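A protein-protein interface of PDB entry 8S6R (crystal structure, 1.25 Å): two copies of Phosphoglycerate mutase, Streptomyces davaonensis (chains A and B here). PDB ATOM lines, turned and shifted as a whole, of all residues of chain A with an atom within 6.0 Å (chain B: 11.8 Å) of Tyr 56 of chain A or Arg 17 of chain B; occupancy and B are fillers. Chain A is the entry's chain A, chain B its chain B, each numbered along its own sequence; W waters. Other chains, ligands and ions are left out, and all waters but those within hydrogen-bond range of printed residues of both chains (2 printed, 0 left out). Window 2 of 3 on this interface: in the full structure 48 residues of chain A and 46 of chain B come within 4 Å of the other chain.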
ATOM      1  N   GLY A  52     -29.103  26.967   5.949  1.00  0.00           N
ATOM      2  CA  GLY A  52     -28.462  26.624   4.697  1.00  0.00           C
ATOM      3  C   GLY A  52     -27.181  25.830   4.824  1.00  0.00           C
ATOM      4  O   GLY A  52     -26.521  25.593   3.804  1.00  0.00           O
ATOM      5  N   LEU A  53     -26.802  25.397   6.034  1.00  0.00           N
ATOM      6  CA  LEU A  53     -25.546  24.663   6.196  1.00  0.00           C
ATOM      7  C   LEU A  53     -25.545  23.333   5.442  1.00  0.00           C
ATOM      8  O   LEU A  53     -24.468  22.848   5.069  1.00  0.00           O
ATOM      9  CB  LEU A  53     -25.223  24.476   7.685  1.00  0.00           C
ATOM     10  CG  LEU A  53     -23.773  24.159   8.093  1.00  0.00           C
ATOM     11  CD1 LEU A  53     -22.757  25.104   7.463  1.00  0.00           C
ATOM     12  CD2 LEU A  53     -23.639  24.217   9.616  1.00  0.00           C
ATOM     13  N   GLU A  54     -26.723  22.751   5.185  1.00  0.00           N
ATOM     14  CA  GLU A  54     -26.792  21.487   4.451  1.00  0.00           C
ATOM     15  C   GLU A  54     -26.240  21.607   3.035  1.00  0.00           C
ATOM     16  O   GLU A  54     -25.699  20.630   2.496  1.00  0.00           O
ATOM     17  CB  GLU A  54     -28.235  20.987   4.396  1.00  0.00           C
ATOM     18  CG  GLU A  54     -28.851  20.702   5.754  1.00  0.00           C
ATOM     19  CD  GLU A  54     -29.657  21.869   6.293  1.00  0.00           C
ATOM     20  OE1 GLU A  54     -29.268  23.040   6.059  1.00  0.00           O
ATOM     21  OE2 GLU A  54     -30.688  21.607   6.951  1.00  0.00           O
ATOM     22  N   ASP A  55     -26.386  22.773   2.404  1.00  0.00           N
ATOM     23  CA  ASP A  55     -25.926  22.983   1.034  1.00  0.00           C
ATOM     24  C   ASP A  55     -24.716  23.906   0.950  1.00  0.00           C
ATOM     25  O   ASP A  55     -24.305  24.274  -0.154  1.00  0.00           O
ATOM     26  CB  ASP A  55     -27.061  23.519   0.160  1.00  0.00           C
ATOM     27  CG  ASP A  55     -28.211  22.542   0.035  1.00  0.00           C
ATOM     28  OD1 ASP A  55     -27.967  21.317   0.115  1.00  0.00           O
ATOM     29  OD2 ASP A  55     -29.359  22.998  -0.149  1.00  0.00           O
ATOM     30  N   TYR A  56     -24.137  24.279   2.089  1.00  0.00           N
ATOM     31  CA  TYR A  56     -23.001  25.195   2.111  1.00  0.00           C
ATOM     32  C   TYR A  56     -21.829  24.623   1.323  1.00  0.00           C
ATOM     33  O   TYR A  56     -21.408  23.484   1.550  1.00  0.00           O
ATOM     34  CB  TYR A  56     -22.573  25.419   3.552  1.00  0.00           C
ATOM     35  CG  TYR A  56     -21.563  26.520   3.733  1.00  0.00           C
ATOM     36  CD1 TYR A  56     -21.851  27.821   3.330  1.00  0.00           C
ATOM     37  CD2 TYR A  56     -20.339  26.272   4.335  1.00  0.00           C
ATOM     38  CE1 TYR A  56     -20.942  28.847   3.516  1.00  0.00           C
ATOM     39  CE2 TYR A  56     -19.409  27.294   4.534  1.00  0.00           C
ATOM     40  CZ  TYR A  56     -19.724  28.584   4.114  1.00  0.00           C
ATOM     41  OH  TYR A  56     -18.845  29.626   4.294  1.00  0.00           O
ATOM     42  N   ASP A  57     -21.287  25.425   0.403  1.00  0.00           N
ATOM     43  CA  ASP A  57     -20.185  25.004  -0.453  1.00  0.00           C
ATOM     44  C   ASP A  57     -18.812  25.481   0.028  1.00  0.00           C
ATOM     45  O   ASP A  57     -17.895  25.642  -0.784  1.00  0.00           O
ATOM     46  CB  ASP A  57     -20.435  25.476  -1.882  1.00  0.00           C
ATOM     47  CG  ASP A  57     -21.465  24.620  -2.614  1.00  0.00           C
ATOM     48  OD1 ASP A  57     -21.661  23.443  -2.230  1.00  0.00           O
ATOM     49  OD2 ASP A  57     -22.076  25.125  -3.584  1.00  0.00           O
ATOM     50  N   GLY A  58     -18.636  25.677   1.324  1.00  0.00           N
ATOM     51  CA  GLY A  58     -17.344  25.994   1.916  1.00  0.00           C
ATOM     52  C   GLY A  58     -16.990  25.004   3.018  1.00  0.00           C
ATOM     53  O   GLY A  58     -17.526  23.891   3.034  1.00  0.00           O
ATOM     54  N   ASP A  59     -16.118  25.374   3.942  1.00  0.00           N
ATOM     55  CA  ASP A  59     -15.783  24.428   5.010  1.00  0.00           C
ATOM     56  C   ASP A  59     -16.993  24.381   5.925  1.00  0.00           C
ATOM     57  O   ASP A  59     -17.275  25.389   6.559  1.00  0.00           O
ATOM     58  CB  ASP A  59     -14.586  25.022   5.765  1.00  0.00           C
ATOM     59  CG  ASP A  59     -14.055  24.105   6.883  1.00  0.00           C
ATOM     60  OD1 ASP A  59     -14.832  23.329   7.453  1.00  0.00           O
ATOM     61  OD2 ASP A  59     -12.832  24.167   7.141  1.00  0.00           O
ATOM     62  N   PRO A  60     -17.729  23.267   6.058  1.00  0.00           N
ATOM     63  CA  PRO A  60     -18.976  23.353   6.845  1.00  0.00           C
ATOM     64  C   PRO A  60     -18.744  23.553   8.330  1.00  0.00           C
ATOM     65  O   PRO A  60     -19.684  23.897   9.060  1.00  0.00           O
ATOM     66  CB  PRO A  60     -19.683  22.028   6.551  1.00  0.00           C
ATOM     67  CG  PRO A  60     -18.592  21.101   6.411  1.00  0.00           C
ATOM     68  CD  PRO A  60     -17.488  21.878   5.628  1.00  0.00           C
ATOM     69  N   ASP A  62     -16.576  25.808   9.403  1.00  0.00           N
ATOM     70  CA  ASP A  62     -16.212  27.210   9.588  1.00  0.00           C
ATOM     71  C   ASP A  62     -16.952  28.083   8.571  1.00  0.00           C
ATOM     72  O   ASP A  62     -16.352  28.788   7.744  1.00  0.00           O
ATOM     73  CB  ASP A  62     -14.702  27.364   9.470  1.00  0.00           C
ATOM     74  CG  ASP A  62     -14.203  28.697   9.958  1.00  0.00           C
ATOM     75  OD1 ASP A  62     -14.943  29.414  10.644  1.00  0.00           O
ATOM     76  OD2 ASP A  62     -13.050  29.038   9.669  1.00  0.00           O
ATOM     77  N   PRO A  63     -18.278  28.110   8.643  1.00  0.00           N
ATOM     78  CA  PRO A  63     -19.064  28.877   7.672  1.00  0.00           C
ATOM     79  C   PRO A  63     -19.103  30.376   7.965  1.00  0.00           C
ATOM     80  O   PRO A  63     -18.955  30.813   9.109  1.00  0.00           O
ATOM     81  CB  PRO A  63     -20.469  28.275   7.831  1.00  0.00           C
ATOM     82  CG  PRO A  63     -20.524  27.858   9.303  1.00  0.00           C
ATOM     83  CD  PRO A  63     -19.116  27.373   9.610  1.00  0.00           C
ATOM     84  N   ALA A  64     -19.393  31.153   6.923  1.00  0.00           N
ATOM     85  CA  ALA A  64     -19.769  32.552   7.079  1.00  0.00           C
ATOM     86  C   ALA A  64     -21.155  32.631   7.720  1.00  0.00           C
ATOM     87  O   ALA A  64     -21.883  31.646   7.795  1.00  0.00           O
ATOM     88  CB  ALA A  64     -19.835  33.243   5.713  1.00  0.00           C
ATOM     89  N   TRP A 124     -18.407  16.095  16.005  1.00  0.00           N
ATOM     90  CA  TRP A 124     -18.219  16.397  14.591  1.00  0.00           C
ATOM     91  C   TRP A 124     -16.772  16.788  14.300  1.00  0.00           C
ATOM     92  O   TRP A 124     -16.195  16.327  13.311  1.00  0.00           O
ATOM     93  CB  TRP A 124     -19.211  17.493  14.177  1.00  0.00           C
ATOM     94  CG  TRP A 124     -19.208  17.825  12.680  1.00  0.00           C
ATOM     95  CD1 TRP A 124     -18.701  17.062  11.659  1.00  0.00           C
ATOM     96  CD2 TRP A 124     -19.744  19.007  12.076  1.00  0.00           C
ATOM     97  NE1 TRP A 124     -18.903  17.710  10.450  1.00  0.00           N
ATOM     98  CE2 TRP A 124     -19.554  18.890  10.688  1.00  0.00           C
ATOM     99  CE3 TRP A 124     -20.395  20.144  12.574  1.00  0.00           C
ATOM    100  CZ2 TRP A 124     -19.945  19.882   9.796  1.00  0.00           C
ATOM    101  CZ3 TRP A 124     -20.794  21.127  11.670  1.00  0.00           C
ATOM    102  CH2 TRP A 124     -20.568  20.983  10.310  1.00  0.00           C
ATOM    103  N   MET B  13     -17.906   7.371   9.303  1.00  0.00           N
ATOM    104  CA  MET B  13     -18.451   7.382   7.924  1.00  0.00           C
ATOM    105  C   MET B  13     -18.098   8.717   7.240  1.00  0.00           C
ATOM    106  O   MET B  13     -17.013   9.194   7.519  1.00  0.00           O
ATOM    107  CB  MET B  13     -19.941   7.019   7.881  1.00  0.00           C
ATOM    108  CG  MET B  13     -20.331   6.106   6.719  1.00  0.00           C
ATOM    109  SD  MET B  13     -20.802   4.385   7.081  1.00  0.00           S
ATOM    110  CE  MET B  13     -20.790   3.720   5.416  1.00  0.00           C
ATOM    111  N   SER B  14     -19.021   9.398   6.557  1.00  0.00           N
ATOM    112  CA  SER B  14     -18.611  10.524   5.672  1.00  0.00           C
ATOM    113  C   SER B  14     -18.626  11.953   6.228  1.00  0.00           C
ATOM    114  O   SER B  14     -17.658  12.361   6.835  1.00  0.00           O
ATOM    115  CB  SER B  14     -19.373  10.462   4.389  1.00  0.00           C
ATOM    116  OG  SER B  14     -18.533  10.878   3.336  1.00  0.00           O
ATOM    117  N   ASP B  15     -19.616  12.736   5.795  1.00  0.00           N
ATOM    118  CA  ASP B  15     -19.789  14.163   6.168  1.00  0.00           C
ATOM    119  C   ASP B  15     -20.768  14.204   7.346  1.00  0.00           C
ATOM    120  O   ASP B  15     -21.930  13.855   7.151  1.00  0.00           O
ATOM    121  CB  ASP B  15     -20.313  14.968   4.970  1.00  0.00           C
ATOM    122  CG  ASP B  15     -20.339  16.472   5.167  1.00  0.00           C
ATOM    123  OD1 ASP B  15     -20.751  16.903   6.228  1.00  0.00           O
ATOM    124  OD2 ASP B  15     -19.994  17.197   4.243  1.00  0.00           O
ATOM    125  N   GLY B  16     -20.305  14.654   8.507  1.00  0.00           N
ATOM    126  CA  GLY B  16     -21.184  14.645   9.686  1.00  0.00           C
ATOM    127  C   GLY B  16     -22.037  15.887   9.832  1.00  0.00           C
ATOM    128  O   GLY B  16     -22.570  16.051  10.905  1.00  0.00           O
ATOM    129  N   ARG B  17     -22.188  16.717   8.806  1.00  0.00           N
ATOM    130  CA  ARG B  17     -22.952  17.947   9.022  1.00  0.00           C
ATOM    131  C   ARG B  17     -24.435  17.666   9.266  1.00  0.00           C
ATOM    132  O   ARG B  17     -25.060  18.332  10.092  1.00  0.00           O
ATOM    133  CB  ARG B  17     -22.737  18.958   7.882  1.00  0.00           C
ATOM    134  CG  ARG B  17     -23.611  18.786   6.643  1.00  0.00           C
ATOM    135  CD  ARG B  17     -23.330  19.874   5.598  1.00  0.00           C
ATOM    136  NE  ARG B  17     -22.069  19.618   4.907  1.00  0.00           N
ATOM    137  CZ  ARG B  17     -21.499  20.438   4.035  1.00  0.00           C
ATOM    138  NH1 ARG B  17     -22.054  21.594   3.704  1.00  0.00           N
ATOM    139  NH2 ARG B  17     -20.360  20.070   3.447  1.00  0.00           N
ATOM    140  N   GLU B  18     -25.022  16.695   8.565  1.00  0.00           N
ATOM    141  CA  GLU B  18     -26.440  16.400   8.783  1.00  0.00           C
ATOM    142  C   GLU B  18     -26.688  15.854  10.184  1.00  0.00           C
ATOM    143  O   GLU B  18     -27.653  16.243  10.841  1.00  0.00           O
ATOM    144  CB  GLU B  18     -26.954  15.438   7.706  1.00  0.00           C
ATOM    145  CG  GLU B  18     -27.042  16.059   6.314  1.00  0.00           C
ATOM    146  CD  GLU B  18     -28.221  17.024   6.150  1.00  0.00           C
ATOM    147  OE1 GLU B  18     -28.911  17.330   7.151  1.00  0.00           O
ATOM    148  OE2 GLU B  18     -28.467  17.473   5.005  1.00  0.00           O
ATOM    149  N   SER B  19     -25.836  14.956  10.656  1.00  0.00           N
ATOM    150  CA  SER B  19     -25.947  14.443  12.021  1.00  0.00           C
ATOM    151  C   SER B  19     -25.855  15.574  13.036  1.00  0.00           C
ATOM    152  O   SER B  19     -26.696  15.704  13.946  1.00  0.00           O
ATOM    153  CB  SER B  19     -24.812  13.430  12.215  1.00  0.00           C
ATOM    154  OG  SER B  19     -24.775  12.943  13.540  1.00  0.00           O
ATOM    155  N   PHE B  20     -24.870  16.453  12.850  1.00  0.00           N
ATOM    156  CA  PHE B  20     -24.731  17.630  13.694  1.00  0.00           C
ATOM    157  C   PHE B  20     -25.996  18.482  13.699  1.00  0.00           C
ATOM    158  O   PHE B  20     -26.472  18.896  14.766  1.00  0.00           O
ATOM    159  CB  PHE B  20     -23.522  18.453  13.237  1.00  0.00           C
ATOM    160  CG  PHE B  20     -23.333  19.719  14.061  1.00  0.00           C
ATOM    161  CD1 PHE B  20     -22.655  19.661  15.271  1.00  0.00           C
ATOM    162  CD2 PHE B  20     -23.826  20.938  13.622  1.00  0.00           C
ATOM    163  CE1 PHE B  20     -22.459  20.796  16.036  1.00  0.00           C
ATOM    164  CE2 PHE B  20     -23.646  22.087  14.385  1.00  0.00           C
ATOM    165  CZ  PHE B  20     -22.961  22.013  15.594  1.00  0.00           C
ATOM    166  N   LEU B  21     -26.555  18.765  12.524  1.00  0.00           N
ATOM    167  CA  LEU B  21     -27.700  19.657  12.480  1.00  0.00           C
ATOM    168  C   LEU B  21     -28.946  18.997  13.020  1.00  0.00           C
ATOM    169  O   LEU B  21     -29.783  19.688  13.630  1.00  0.00           O
ATOM    170  CB  LEU B  21     -27.938  20.131  11.057  1.00  0.00           C
ATOM    171  CG  LEU B  21     -26.828  20.978  10.441  1.00  0.00           C
ATOM    172  CD1 LEU B  21     -27.127  21.171   8.963  1.00  0.00           C
ATOM    173  CD2 LEU B  21     -26.698  22.306  11.120  1.00  0.00           C
ATOM    174  N   GLU B  22     -29.089  17.690  12.843  1.00  0.00           N
ATOM    175  CA  GLU B  22     -30.236  16.992  13.427  1.00  0.00           C
ATOM    176  C   GLU B  22     -30.181  17.063  14.948  1.00  0.00           C
ATOM    177  O   GLU B  22     -31.191  17.338  15.602  1.00  0.00           O
ATOM    178  CB  GLU B  22     -30.258  15.538  12.962  1.00  0.00           C
ATOM    179  CG  GLU B  22     -31.515  14.771  13.349  1.00  0.00           C
ATOM    180  CD  GLU B  22     -31.812  13.628  12.383  1.00  0.00           C
ATOM    181  OE1 GLU B  22     -30.934  13.301  11.549  1.00  0.00           O
ATOM    182  OE2 GLU B  22     -32.927  13.062  12.445  1.00  0.00           O
ATOM    183  N   VAL B  23     -29.000  16.849  15.533  1.00  0.00           N
ATOM    184  CA  VAL B  23     -28.872  16.963  16.987  1.00  0.00           C
ATOM    185  C   VAL B  23     -29.090  18.407  17.441  1.00  0.00           C
ATOM    186  O   VAL B  23     -29.831  18.667  18.415  1.00  0.00           O
ATOM    187  CB  VAL B  23     -27.516  16.399  17.434  1.00  0.00           C
ATOM    188  CG1 VAL B  23     -27.295  16.698  18.936  1.00  0.00           C
ATOM    189  CG2 VAL B  23     -27.494  14.956  17.234  1.00  0.00           C
ATOM    190  N   MET B  24     -28.510  19.375  16.722  1.00  0.00           N
ATOM    191  CA  MET B  24     -28.684  20.781  17.070  1.00  0.00           C
ATOM    192  C   MET B  24     -30.162  21.160  17.095  1.00  0.00           C
ATOM    193  O   MET B  24     -30.610  21.877  17.994  1.00  0.00           O
ATOM    194  CB  MET B  24     -27.948  21.671  16.073  1.00  0.00           C
ATOM    195  CG  MET B  24     -27.986  23.144  16.446  1.00  0.00           C
ATOM    196  SD  MET B  24     -27.257  24.196  15.217  1.00  0.00           S
ATOM    197  CE  MET B  24     -28.453  24.048  13.893  1.00  0.00           C
ATOM    198  N   ARG B  25     -30.938  20.687  16.118  1.00  0.00           N
ATOM    199  CA  ARG B  25     -32.367  20.984  16.095  1.00  0.00           C
ATOM    200  C   ARG B  25     -33.074  20.324  17.268  1.00  0.00           C
ATOM    201  O   ARG B  25     -33.965  20.926  17.880  1.00  0.00           O
ATOM    202  CB  ARG B  25     -32.934  20.521  14.758  1.00  0.00           C
ATOM    203  CG  ARG B  25     -34.407  20.784  14.543  1.00  0.00           C
ATOM    204  CD  ARG B  25     -34.818  20.424  13.092  1.00  0.00           C
ATOM    205  NE  ARG B  25     -33.892  19.512  12.410  1.00  0.00           N
ATOM    206  CZ  ARG B  25     -33.092  19.843  11.397  1.00  0.00           C
ATOM    207  NH1 ARG B  25     -33.043  21.080  10.926  1.00  0.00           N
ATOM    208  NH2 ARG B  25     -32.330  18.905  10.832  1.00  0.00           N
ATOM    209  N   SER B  26     -32.685  19.101  17.618  1.00  0.00           N
ATOM    210  CA  SER B  26     -33.312  18.403  18.734  1.00  0.00           C
ATOM    211  C   SER B  26     -33.036  19.124  20.053  1.00  0.00           C
ATOM    212  O   SER B  26     -33.927  19.240  20.912  1.00  0.00           O
ATOM    213  CB  SER B  26     -32.805  16.965  18.794  1.00  0.00           C
ATOM    214  OG  SER B  26     -33.323  16.230  17.702  1.00  0.00           O
HETATM  215  O   HOH W   1     -19.203  21.987   1.806  1.00  0.00           O
HETATM  216  O   HOH W   2     -18.400  17.495   7.636  1.00  0.00           O
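Water W1 lies within hydrogen-bond range of the backbone carbonyl oxygen of Tyr 56 of chain A (2.7 Å), the guanidinium group of Arg 17 of chain B (2.8 Å) and the backbone carbonyl oxygen of Gly 58 of chain A (2.8 Å). Water W2 lies within hydrogen-bond range of the side-chain carboxylate of Asp 15 of chain B (2.8 Å) and the indole nitrogen of Trp 124 of chain A (2.9 Å).
Leu 53 of chain A touches Leu 21 of chain B (CD2 to CD2, 3.9 Å). NH1 of Arg 17 of chain B touches O of Glu 54 of chain A (3.96 Å). CG of Glu 54 of chain A touches OE2 of Glu 18 of chain B, 3.3 Å away. Leu 21 of chain B touches Glu 54 of chain A. Pro 60 of chain A touches Arg 17 of chain B (CB to CZ, 3.5 Å). Trp 124 of chain A touches Gly 16 of chain B. Trp 124 of chain A touches Arg 17 of chain B. Phe 20 of chain B touches Trp 124 of chain A (CG to CE3, 3.3 Å).
The backbone carbonyl oxygen (O) of Leu 53 of chain A sits at hydrogen-bond distance from the guanidinium group (NH1) of Arg 17 of chain B (3.0 Å). The backbone carbonyl oxygen (O) of Tyr 56 of chain A sits at hydrogen-bond distance from the guanidinium group (NH1) of Arg 17 of chain B (2.9 Å).
Of chain B, only Arg 17 (2.9 Å) comes within 4 Å of Tyr 56 of chain A. Arg 17 of chain B touches just these residues of chain A: Leu 53, Glu 54, Tyr 56, Pro 60 and Trp 124. Of chain B, only Arg 17 and Leu 21 come within 4 Å of Leu 53 of chain A. Of chain B, only Arg 17 (3.96 Å), Glu 18 (3.3 Å) and Leu 21 (3.7 Å) come within 4 Å of Glu 54 of chain A. No residue of chain B comes within 4 Å of Asp 55 of chain A. No residue of chain B comes within 4 Å of Gly 58 of chain A. No residue of chain B comes within 4 Å of Asp 59 of chain A. Printed residues of chain B within 4 Å of Pro 60 of chain A: Arg 17. No residue of chain B comes within 4 Å of Ala 64 of chain A. Of the printed residues of chain A, Leu 21 of chain B touches Leu 53 and Glu 54. Of the printed residues of chain A, Glu 18 of chain B touches Glu 54. Printed residues of chain A within 4 Å of Gly 16 of chain B: Trp 124. Of the printed residues of chain B, Trp 124 of chain A touches Gly 16 (3.7 Å), Arg 17 (3.5 Å) and Phe 20 (3.3 Å). Ser 26 of chain B touches none of the printed residues of chain A. The nearest residue of chain B that does not touch Tyr 56 of chain A is Asp 15 of chain B (7.0 Å). The nearest printed residue of chain A that does not touch Phe 20 of chain B is Leu 53 of chain A (5.2 Å).
The side-chain hydroxyl of Tyr 56 of chain A lies within hydrogen-bond range of the backbone NH of Ala 64 of chain A. NH2 of Arg 17 of chain B lies within salt-bridge range of OD2 of Asp 15 of chain B, at 3.0 Å.
Hydrophobic or aromatic side chains of chain A that line the printed part of chain B: Leu 53, Tyr 56, Pro 60 and Trp 124. Hydrophobic or aromatic side chains of chain B that line the printed part of chain A: Phe 20 and Leu 21. Among the printed residues, no Asp or Glu carboxylate lies within 4 Å of a Lys or Arg side-chain nitrogen of the other chain.
No position is printed for both chains. Of the 10 pairs that touch across the chains among the printed residues, none has its exchanged pair printed and touching as well.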
